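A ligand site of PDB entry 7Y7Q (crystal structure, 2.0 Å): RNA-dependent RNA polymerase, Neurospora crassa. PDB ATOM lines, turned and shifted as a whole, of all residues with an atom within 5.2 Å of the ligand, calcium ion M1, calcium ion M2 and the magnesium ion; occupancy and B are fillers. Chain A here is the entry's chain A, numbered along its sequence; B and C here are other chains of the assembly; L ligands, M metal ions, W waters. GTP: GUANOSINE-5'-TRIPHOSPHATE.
The side-chain amino group (NZ) of Lys 391 lies within salt-bridge range of an oxygen (O2G) of the ligand, 3.4 Å away.
O2G of the ligand is in salt-bridge range of NH2 of Arg 295.
A nitrogen (N2) of the ligand is in hydrogen-bond range of O2 of C 7 of chain B (2.8 Å).
The side-chain amino group (NZ) of Lys 743 lies within salt-bridge range of an oxygen (O1G) of the ligand, at 3.0 Å.
O2 of C 8 of chain B sits close to a nitrogen (N2) of the ligand (3.3 Å).
An oxygen (O2') of the ligand sits at hydrogen-bond distance from the guanidinium group of Arg 586 (2.9 Å).
NE of Arg 586 lies within salt-bridge range of OD2 of Asp 635 (3.2 Å).
O2' of G 7 of chain C sits at hydrogen-bond distance from NH2 of Arg 586 (3.3 Å).
The guanidinium group of Arg 586 is in hydrogen-bond range of the backbone carbonyl oxygen of Ser 628 (3.0 Å).
OP1 of G 7 of chain C is in salt-bridge range of the side-chain amino group (NZ) of Lys 367.
OG of Ser 628 lies within hydrogen-bond range of O of Pro 588 (2.7 Å).
O6 of G 7 of chain C sits close to O6 of the ligand.
Residues that only touch the ligand: Pro 588 (3.6 Å), Val 739 (3.3 Å) and Asp 740 (3.6 Å).
The nearest printed residue that does not touch the ligand is Asp 635 (4.1 Å).
Of the 20 residues printed, 3 come within 4 Å of calcium ion M1.
The nearest printed residue that does not touch calcium ion M1 is G 7 of chain C (4.4 Å).
Two residues have an atom within 4 Å of calcium ion M2: Asp 631 and Asp 633.
The nearest printed residue that does not touch calcium ion M2 is Asp 333 (4.1 Å).
Residues that only touch the magnesium ion: Gly 629 (2.9 Å).
Within 4 Å of the magnesium ion: Gly 629 and Asp 631.
The nearest printed residue that does not touch the magnesium ion is Gly 630 (4.2 Å).
Calcium ion M1 is bound by water W5 (2.3 Å), OD1 of Asp 631 (2.4 Å), OD1 of Asp 633 (2.5 Å), O2A of the ligand (2.6 Å), O2B of the ligand (2.7 Å), OD1 of Asp 635 (2.7 Å), OD2 of Asp 633 (2.8 Å) and OD2 of Asp 631 (2.8 Å).
O3G of the ligand binds calcium ion M2, at 2.1 Å.
Water W10 binds calcium ion M2, at 2.3 Å.
Calcium ion M2 is bound by O2B of the ligand.
Water W3 is bound to calcium ion M2, 2.4 Å away.
Calcium ion M2 is bound by the side-chain carboxylate (OD2) of Asp 631, at 2.4 Å.
Calcium ion M2 is bound by OD2 of Asp 633.
The magnesium ion is bound by the side-chain carboxylate of Asp 631 (2.5 Å).
Water W5 bridges OD2 of Asp 635 (2.7 Å) and O5' of the ligand (3.4 Å).
Water W1 lies within hydrogen-bond range of O of Asp 633 (3.0 Å), OP1 of G 7 of chain C (3.1 Å) and NZ of Lys 367 (3.4 Å).
Water W6 bridges an oxygen (O2') of the ligand (2.8 Å) and the backbone carbonyl oxygen of Ser 628 (3.3 Å).
Water W8 bridges O6 of G 7 of chain C (2.7 Å) and an oxygen (O6) of the ligand (3.0 Å).
Water W4 lies within hydrogen-bond range of the side-chain amino group (NZ) of Lys 367 (2.5 Å), the side-chain amino group (NZ) of Lys 743 (2.9 Å) and an oxygen (O1G) of the ligand (3.0 Å).
Water W7 lies within hydrogen-bond range of OD1 of Asp 333 (2.7 Å) and NZ of Lys 391 (3.4 Å).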
ATOM      1  N   ARG A 295      13.445 -21.314   7.235  1.00  0.00           N
ATOM      2  CA  ARG A 295      13.695 -22.625   7.832  1.00  0.00           C
ATOM      3  C   ARG A 295      15.154 -22.845   8.182  1.00  0.00           C
ATOM      4  O   ARG A 295      15.466 -23.819   8.884  1.00  0.00           O
ATOM      5  CB  ARG A 295      13.200 -23.734   6.902  1.00  0.00           C
ATOM      6  CG  ARG A 295      11.714 -23.632   6.577  1.00  0.00           C
ATOM      7  CD  ARG A 295      10.906 -23.413   7.842  1.00  0.00           C
ATOM      8  NE  ARG A 295       9.471 -23.386   7.583  1.00  0.00           N
ATOM      9  CZ  ARG A 295       8.554 -23.142   8.512  1.00  0.00           C
ATOM     10  NH1 ARG A 295       8.890 -22.887   9.759  1.00  0.00           N
ATOM     11  NH2 ARG A 295       7.268 -23.150   8.170  1.00  0.00           N
ATOM     12  N   ASP A 333      -1.548 -30.235  14.767  1.00  0.00           N
ATOM     13  CA  ASP A 333      -0.515 -29.406  14.088  1.00  0.00           C
ATOM     14  C   ASP A 333       0.695 -29.204  15.000  1.00  0.00           C
ATOM     15  O   ASP A 333       0.555 -28.515  16.003  1.00  0.00           O
ATOM     16  CB  ASP A 333      -1.143 -28.088  13.622  1.00  0.00           C
ATOM     17  CG  ASP A 333      -0.232 -27.187  12.807  1.00  0.00           C
ATOM     18  OD1 ASP A 333       0.891 -27.587  12.516  1.00  0.00           O
ATOM     19  OD2 ASP A 333      -0.678 -26.075  12.484  1.00  0.00           O
ATOM     20  N   LYS A 367       9.807 -30.055  13.373  1.00  0.00           N
ATOM     21  CA  LYS A 367       9.923 -29.250  14.580  1.00  0.00           C
ATOM     22  C   LYS A 367       8.565 -29.192  15.258  1.00  0.00           C
ATOM     23  O   LYS A 367       7.519 -29.261  14.609  1.00  0.00           O
ATOM     24  CB  LYS A 367      10.427 -27.829  14.275  1.00  0.00           C
ATOM     25  CG  LYS A 367       9.394 -26.905  13.675  1.00  0.00           C
ATOM     26  CD  LYS A 367       9.136 -25.724  14.604  1.00  0.00           C
ATOM     27  CE  LYS A 367      10.398 -24.928  14.838  1.00  0.00           C
ATOM     28  NZ  LYS A 367      10.125 -23.548  15.333  1.00  0.00           N
ATOM     29  N   LYS A 391       8.951 -29.205   7.959  1.00  0.00           N
ATOM     30  CA  LYS A 391       8.994 -27.913   7.291  1.00  0.00           C
ATOM     31  C   LYS A 391       9.685 -27.960   5.931  1.00  0.00           C
ATOM     32  O   LYS A 391       9.688 -26.943   5.220  1.00  0.00           O
ATOM     33  CB  LYS A 391       9.690 -26.887   8.190  1.00  0.00           C
ATOM     34  CG  LYS A 391       9.021 -26.714   9.545  1.00  0.00           C
ATOM     35  CD  LYS A 391       7.498 -26.705   9.411  1.00  0.00           C
ATOM     36  CE  LYS A 391       6.829 -26.377  10.737  1.00  0.00           C
ATOM     37  NZ  LYS A 391       5.354 -26.294  10.603  1.00  0.00           N
ATOM     38  N   ARG A 586      -3.482 -17.541  24.472  1.00  0.00           N
ATOM     39  CA  ARG A 586      -2.081 -17.362  24.136  1.00  0.00           C
ATOM     40  C   ARG A 586      -1.745 -15.872  24.157  1.00  0.00           C
ATOM     41  O   ARG A 586      -2.607 -15.020  23.930  1.00  0.00           O
ATOM     42  CB  ARG A 586      -1.744 -17.940  22.759  1.00  0.00           C
ATOM     43  CG  ARG A 586      -1.631 -19.455  22.712  1.00  0.00           C
ATOM     44  CD  ARG A 586      -1.215 -19.933  21.318  1.00  0.00           C
ATOM     45  NE  ARG A 586       0.039 -19.332  20.883  1.00  0.00           N
ATOM     46  CZ  ARG A 586       0.189 -18.618  19.770  1.00  0.00           C
ATOM     47  NH1 ARG A 586      -0.821 -18.402  18.952  1.00  0.00           N
ATOM     48  NH2 ARG A 586       1.392 -18.123  19.485  1.00  0.00           N
ATOM     49  N   SER A 587      -0.482 -15.579  24.429  1.00  0.00           N
ATOM     50  CA  SER A 587       0.004 -14.227  24.197  1.00  0.00           C
ATOM     51  C   SER A 587       0.693 -14.181  22.845  1.00  0.00           C
ATOM     52  O   SER A 587       1.486 -15.071  22.533  1.00  0.00           O
ATOM     53  CB  SER A 587       0.992 -13.818  25.293  1.00  0.00           C
ATOM     54  OG  SER A 587       0.577 -14.301  26.557  1.00  0.00           O
ATOM     55  N   PRO A 588       0.419 -13.156  22.010  1.00  0.00           N
ATOM     56  CA  PRO A 588      -0.467 -12.031  22.304  1.00  0.00           C
ATOM     57  C   PRO A 588      -1.933 -12.335  22.029  1.00  0.00           C
ATOM     58  O   PRO A 588      -2.254 -13.033  21.061  1.00  0.00           O
ATOM     59  CB  PRO A 588       0.039 -10.955  21.352  1.00  0.00           C
ATOM     60  CG  PRO A 588       0.470 -11.729  20.143  1.00  0.00           C
ATOM     61  CD  PRO A 588       1.014 -13.045  20.669  1.00  0.00           C
ATOM     62  N   SER A 628      -5.375 -17.196  19.130  1.00  0.00           N
ATOM     63  CA  SER A 628      -4.475 -16.350  18.346  1.00  0.00           C
ATOM     64  C   SER A 628      -3.747 -17.162  17.271  1.00  0.00           C
ATOM     65  O   SER A 628      -2.556 -16.978  17.032  1.00  0.00           O
ATOM     66  CB  SER A 628      -3.462 -15.642  19.258  1.00  0.00           C
ATOM     67  OG  SER A 628      -4.097 -14.679  20.070  1.00  0.00           O
ATOM     68  N   GLY A 629      -4.481 -18.067  16.633  1.00  0.00           N
ATOM     69  CA  GLY A 629      -3.904 -18.901  15.584  1.00  0.00           C
ATOM     70  C   GLY A 629      -2.881 -19.897  16.071  1.00  0.00           C
ATOM     71  O   GLY A 629      -1.936 -20.211  15.338  1.00  0.00           O
ATOM     72  N   GLY A 630      -3.053 -20.423  17.285  1.00  0.00           N
ATOM     73  CA  GLY A 630      -2.068 -21.301  17.875  1.00  0.00           C
ATOM     74  C   GLY A 630      -2.087 -22.721  17.338  1.00  0.00           C
ATOM     75  O   GLY A 630      -2.919 -23.102  16.515  1.00  0.00           O
ATOM     76  N   ASP A 631      -1.138 -23.512  17.818  1.00  0.00           N
ATOM     77  CA  ASP A 631      -1.016 -24.906  17.427  1.00  0.00           C
ATOM     78  C   ASP A 631      -0.276 -25.633  18.552  1.00  0.00           C
ATOM     79  O   ASP A 631      -0.206 -25.137  19.680  1.00  0.00           O
ATOM     80  CB  ASP A 631      -0.300 -25.026  16.079  1.00  0.00           C
ATOM     81  CG  ASP A 631       0.986 -24.229  16.017  1.00  0.00           C
ATOM     82  OD1 ASP A 631       1.709 -24.197  17.033  1.00  0.00           O
ATOM     83  OD2 ASP A 631       1.265 -23.625  14.961  1.00  0.00           O
ATOM     84  N   ASP A 633       3.064 -26.895  18.501  1.00  0.00           N
ATOM     85  CA  ASP A 633       4.461 -27.022  18.103  1.00  0.00           C
ATOM     86  C   ASP A 633       5.410 -26.315  19.073  1.00  0.00           C
ATOM     87  O   ASP A 633       6.538 -25.978  18.706  1.00  0.00           O
ATOM     88  CB  ASP A 633       4.648 -26.487  16.674  1.00  0.00           C
ATOM     89  CG  ASP A 633       4.510 -24.965  16.589  1.00  0.00           C
ATOM     90  OD1 ASP A 633       4.362 -24.303  17.636  1.00  0.00           O
ATOM     91  OD2 ASP A 633       4.541 -24.432  15.457  1.00  0.00           O
ATOM     92  N   ASP A 635       3.762 -23.836  21.268  1.00  0.00           N
ATOM     93  CA  ASP A 635       2.891 -22.828  21.853  1.00  0.00           C
ATOM     94  C   ASP A 635       2.592 -23.182  23.309  1.00  0.00           C
ATOM     95  O   ASP A 635       2.471 -24.358  23.673  1.00  0.00           O
ATOM     96  CB  ASP A 635       1.583 -22.713  21.071  1.00  0.00           C
ATOM     97  CG  ASP A 635       1.766 -22.085  19.706  1.00  0.00           C
ATOM     98  OD1 ASP A 635       2.934 -21.902  19.285  1.00  0.00           O
ATOM     99  OD2 ASP A 635       0.749 -21.802  19.038  1.00  0.00           O
ATOM    100  N   LEU A 706       5.468  -4.086  13.176  1.00  0.00           N
ATOM    101  CA  LEU A 706       4.714  -4.777  14.219  1.00  0.00           C
ATOM    102  C   LEU A 706       4.569  -3.899  15.464  1.00  0.00           C
ATOM    103  O   LEU A 706       3.475  -3.781  16.024  1.00  0.00           O
ATOM    104  CB  LEU A 706       5.399  -6.094  14.571  1.00  0.00           C
ATOM    105  CG  LEU A 706       4.765  -6.857  15.736  1.00  0.00           C
ATOM    106  CD1 LEU A 706       3.319  -7.213  15.409  1.00  0.00           C
ATOM    107  CD2 LEU A 706       5.566  -8.106  16.080  1.00  0.00           C
ATOM    108  N   VAL A 739       3.286 -10.374  12.533  1.00  0.00           N
ATOM    109  CA  VAL A 739       4.159 -11.217  13.343  1.00  0.00           C
ATOM    110  C   VAL A 739       4.735 -12.353  12.503  1.00  0.00           C
ATOM    111  O   VAL A 739       5.894 -12.741  12.670  1.00  0.00           O
ATOM    112  CB  VAL A 739       3.426 -11.729  14.590  1.00  0.00           C
ATOM    113  CG1 VAL A 739       2.303 -12.682  14.198  1.00  0.00           C
ATOM    114  CG2 VAL A 739       4.405 -12.387  15.550  1.00  0.00           C
ATOM    115  N   ASP A 740       3.928 -12.902  11.586  1.00  0.00           N
ATOM    116  CA  ASP A 740       4.351 -13.989  10.701  1.00  0.00           C
ATOM    117  C   ASP A 740       4.999 -13.478   9.415  1.00  0.00           C
ATOM    118  O   ASP A 740       4.975 -14.181   8.403  1.00  0.00           O
ATOM    119  CB  ASP A 740       3.159 -14.879  10.360  1.00  0.00           C
ATOM    120  CG  ASP A 740       2.323 -15.255  11.575  1.00  0.00           C
ATOM    121  OD1 ASP A 740       2.882 -15.841  12.522  1.00  0.00           O
ATOM    122  OD2 ASP A 740       1.117 -14.951  11.578  1.00  0.00           O
ATOM    123  N   LYS A 743       8.101 -15.415   7.644  1.00  0.00           N
ATOM    124  CA  LYS A 743       7.708 -16.751   7.216  1.00  0.00           C
ATOM    125  C   LYS A 743       6.686 -16.696   6.087  1.00  0.00           C
ATOM    126  O   LYS A 743       6.723 -17.530   5.168  1.00  0.00           O
ATOM    127  CB  LYS A 743       7.154 -17.543   8.393  1.00  0.00           C
ATOM    128  CG  LYS A 743       7.632 -18.981   8.464  1.00  0.00           C
ATOM    129  CD  LYS A 743       7.327 -19.600   9.816  1.00  0.00           C
ATOM    130  CE  LYS A 743       8.361 -19.175  10.855  1.00  0.00           C
ATOM    131  NZ  LYS A 743       8.035 -19.699  12.216  1.00  0.00           N
ATOM    132  P     C B   7       8.285  -1.496  20.496  1.00  0.00           P
ATOM    133  OP1   C B   7       8.251  -0.454  21.534  1.00  0.00           O
ATOM    134  OP2   C B   7       9.508  -2.301  20.323  1.00  0.00           O
ATOM    135  O5'   C B   7       7.078  -2.488  20.770  1.00  0.00           O
ATOM    136  C5'   C B   7       5.743  -1.994  20.908  1.00  0.00           C
ATOM    137  C4'   C B   7       4.808  -3.129  21.200  1.00  0.00           C
ATOM    138  O4'   C B   7       4.741  -3.987  20.024  1.00  0.00           O
ATOM    139  C3'   C B   7       5.254  -4.072  22.306  1.00  0.00           C
ATOM    140  O3'   C B   7       4.937  -3.611  23.610  1.00  0.00           O
ATOM    141  C2'   C B   7       4.491  -5.339  21.944  1.00  0.00           C
ATOM    142  O2'   C B   7       3.134  -5.294  22.315  1.00  0.00           O
ATOM    143  C1'   C B   7       4.610  -5.339  20.426  1.00  0.00           C
ATOM    144  N1    C B   7       5.756  -6.086  19.920  1.00  0.00           N
ATOM    145  C2    C B   7       5.663  -7.477  19.833  1.00  0.00           C
ATOM    146  O2    C B   7       4.606  -8.026  20.186  1.00  0.00           O
ATOM    147  N3    C B   7       6.717  -8.194  19.374  1.00  0.00           N
ATOM    148  C4    C B   7       7.829  -7.565  18.999  1.00  0.00           C
ATOM    149  N4    C B   7       8.843  -8.299  18.553  1.00  0.00           N
ATOM    150  C5    C B   7       7.965  -6.149  19.081  1.00  0.00           C
ATOM    151  C6    C B   7       6.908  -5.453  19.534  1.00  0.00           C
ATOM    152  P     C B   8       5.730  -4.163  24.877  1.00  0.00           P
ATOM    153  OP1   C B   8       5.451  -3.282  26.017  1.00  0.00           O
ATOM    154  OP2   C B   8       7.135  -4.411  24.472  1.00  0.00           O
ATOM    155  O5'   C B   8       5.060  -5.584  25.145  1.00  0.00           O
ATOM    156  C5'   C B   8       3.731  -5.652  25.657  1.00  0.00           C
ATOM    157  C4'   C B   8       3.148  -7.032  25.444  1.00  0.00           C
ATOM    158  O4'   C B   8       3.378  -7.472  24.080  1.00  0.00           O
ATOM    159  C3'   C B   8       3.745  -8.149  26.262  1.00  0.00           C
ATOM    160  O3'   C B   8       3.291  -8.151  27.606  1.00  0.00           O
ATOM    161  C2'   C B   8       3.280  -9.371  25.485  1.00  0.00           C
ATOM    162  O2'   C B   8       1.924  -9.690  25.710  1.00  0.00           O
ATOM    163  C1'   C B   8       3.452  -8.884  24.051  1.00  0.00           C
ATOM    164  N1    C B   8       4.740  -9.275  23.454  1.00  0.00           N
ATOM    165  C2    C B   8       4.916 -10.590  23.028  1.00  0.00           C
ATOM    166  O2    C B   8       3.970 -11.386  23.148  1.00  0.00           O
ATOM    167  N3    C B   8       6.091 -10.963  22.480  1.00  0.00           N
ATOM    168  C4    C B   8       7.075 -10.077  22.362  1.00  0.00           C
ATOM    169  N4    C B   8       8.216 -10.483  21.812  1.00  0.00           N
ATOM    170  C5    C B   8       6.934  -8.724  22.799  1.00  0.00           C
ATOM    171  C6    C B   8       5.755  -8.378  23.332  1.00  0.00           C
ATOM    172  P     G C   7      10.342 -21.319  18.577  1.00  0.00           P
ATOM    173  OP1   G C   7      10.002 -22.593  17.871  1.00  0.00           O
ATOM    174  OP2   G C   7      10.909 -20.233  17.703  1.00  0.00           O
ATOM    175  O5'   G C   7       9.038 -20.747  19.324  1.00  0.00           O
ATOM    176  C5'   G C   7       8.107 -21.685  19.920  1.00  0.00           C
ATOM    177  C4'   G C   7       6.857 -20.953  20.332  1.00  0.00           C
ATOM    178  O4'   G C   7       7.204 -19.896  21.259  1.00  0.00           O
ATOM    179  C3'   G C   7       6.088 -20.238  19.225  1.00  0.00           C
ATOM    180  C2'   G C   7       5.307 -19.184  20.019  1.00  0.00           C
ATOM    181  O2'   G C   7       4.123 -19.712  20.565  1.00  0.00           O
ATOM    182  C1'   G C   7       6.293 -18.818  21.128  1.00  0.00           C
ATOM    183  N9    G C   7       7.051 -17.596  20.900  1.00  0.00           N
ATOM    184  C8    G C   7       8.293 -17.500  20.321  1.00  0.00           C
ATOM    185  N7    G C   7       8.748 -16.284  20.265  1.00  0.00           N
ATOM    186  C5    G C   7       7.745 -15.520  20.853  1.00  0.00           C
ATOM    187  C6    G C   7       7.684 -14.119  21.080  1.00  0.00           C
ATOM    188  O6    G C   7       8.523 -13.260  20.787  1.00  0.00           O
ATOM    189  N1    G C   7       6.497 -13.758  21.700  1.00  0.00           N
ATOM    190  C2    G C   7       5.492 -14.631  22.056  1.00  0.00           C
ATOM    191  N2    G C   7       4.420 -14.095  22.661  1.00  0.00           N
ATOM    192  N3    G C   7       5.554 -15.945  21.857  1.00  0.00           N
ATOM    193  C4    G C   7       6.700 -16.317  21.242  1.00  0.00           C
HETATM  194  PG  GTP L   1       5.364 -22.724  11.499  1.00  0.00           P
HETATM  195  O1G GTP L   1       6.765 -22.370  11.867  1.00  0.00           O
HETATM  196  O2G GTP L   1       5.189 -22.939  10.047  1.00  0.00           O
HETATM  197  O3G GTP L   1       4.828 -23.849  12.319  1.00  0.00           O
HETATM  198  O3B GTP L   1       4.478 -21.442  11.849  1.00  0.00           O
HETATM  199  PB  GTP L   1       3.950 -20.834  13.220  1.00  0.00           P
HETATM  200  O1B GTP L   1       3.282 -19.546  12.938  1.00  0.00           O
HETATM  201  O2B GTP L   1       3.222 -21.873  13.978  1.00  0.00           O
HETATM  202  O3A GTP L   1       5.322 -20.542  13.977  1.00  0.00           O
HETATM  203  PA  GTP L   1       5.673 -20.292  15.514  1.00  0.00           P
HETATM  204  O1A GTP L   1       6.908 -19.481  15.608  1.00  0.00           O
HETATM  205  O2A GTP L   1       5.607 -21.580  16.242  1.00  0.00           O
HETATM  206  O5' GTP L   1       4.429 -19.389  15.938  1.00  0.00           O
HETATM  207  C5' GTP L   1       4.462 -17.985  15.605  1.00  0.00           C
HETATM  208  C4' GTP L   1       3.585 -17.254  16.591  1.00  0.00           C
HETATM  209  O4' GTP L   1       4.362 -16.968  17.784  1.00  0.00           O
HETATM  210  C3' GTP L   1       3.043 -15.894  16.136  1.00  0.00           C
HETATM  211  C2' GTP L   1       2.823 -15.200  17.484  1.00  0.00           C
HETATM  212  O2' GTP L   1       1.612 -15.560  18.097  1.00  0.00           O
HETATM  213  C1' GTP L   1       4.039 -15.689  18.279  1.00  0.00           C
HETATM  214  N9  GTP L   1       5.210 -14.835  18.138  1.00  0.00           N
HETATM  215  C8  GTP L   1       6.418 -15.168  17.586  1.00  0.00           C
HETATM  216  N7  GTP L   1       7.273 -14.185  17.583  1.00  0.00           N
HETATM  217  C5  GTP L   1       6.588 -13.129  18.166  1.00  0.00           C
HETATM  218  C6  GTP L   1       7.012 -11.805  18.441  1.00  0.00           C
HETATM  219  O6  GTP L   1       8.110 -11.287  18.197  1.00  0.00           O
HETATM  220  N1  GTP L   1       5.999 -11.062  19.052  1.00  0.00           N
HETATM  221  C2  GTP L   1       4.750 -11.538  19.356  1.00  0.00           C
HETATM  222  N2  GTP L   1       3.906 -10.674  19.939  1.00  0.00           N
HETATM  223  N3  GTP L   1       4.347 -12.778  19.107  1.00  0.00           N
HETATM  224  C4  GTP L   1       5.322 -13.518  18.515  1.00  0.00           C
HETATM  225 CA    CA M   1       3.153 -22.298  16.632  1.00  0.00          CA
HETATM  226 CA    CA M   2       3.072 -24.232  13.462  1.00  0.00          CA
HETATM  227 MG    MG M   3       0.222 -21.542  14.014  1.00  0.00          MG
HETATM  228  O   HOH W   1       7.213 -23.586  17.106  1.00  0.00           O
HETATM  229  O   HOH W   2      -2.713 -22.462  13.829  1.00  0.00           O
HETATM  230  O   HOH W   3       3.158 -26.653  13.437  1.00  0.00           O
HETATM  231  O   HOH W   4       8.771 -21.883  14.042  1.00  0.00           O
HETATM  232  O   HOH W   5       1.401 -20.884  16.580  1.00  0.00           O
HETATM  233  O   HOH W   6      -0.555 -14.379  16.794  1.00  0.00           O
HETATM  234  O   HOH W   7       1.959 -25.827  10.786  1.00  0.00           O
HETATM  235  O   HOH W   8      10.512 -12.779  19.074  1.00  0.00           O
HETATM  236  O   HOH W   9       1.173 -18.535  14.072  1.00  0.00           O
HETATM  237  O   HOH W  10       1.209 -23.867  12.091  1.00  0.00           O
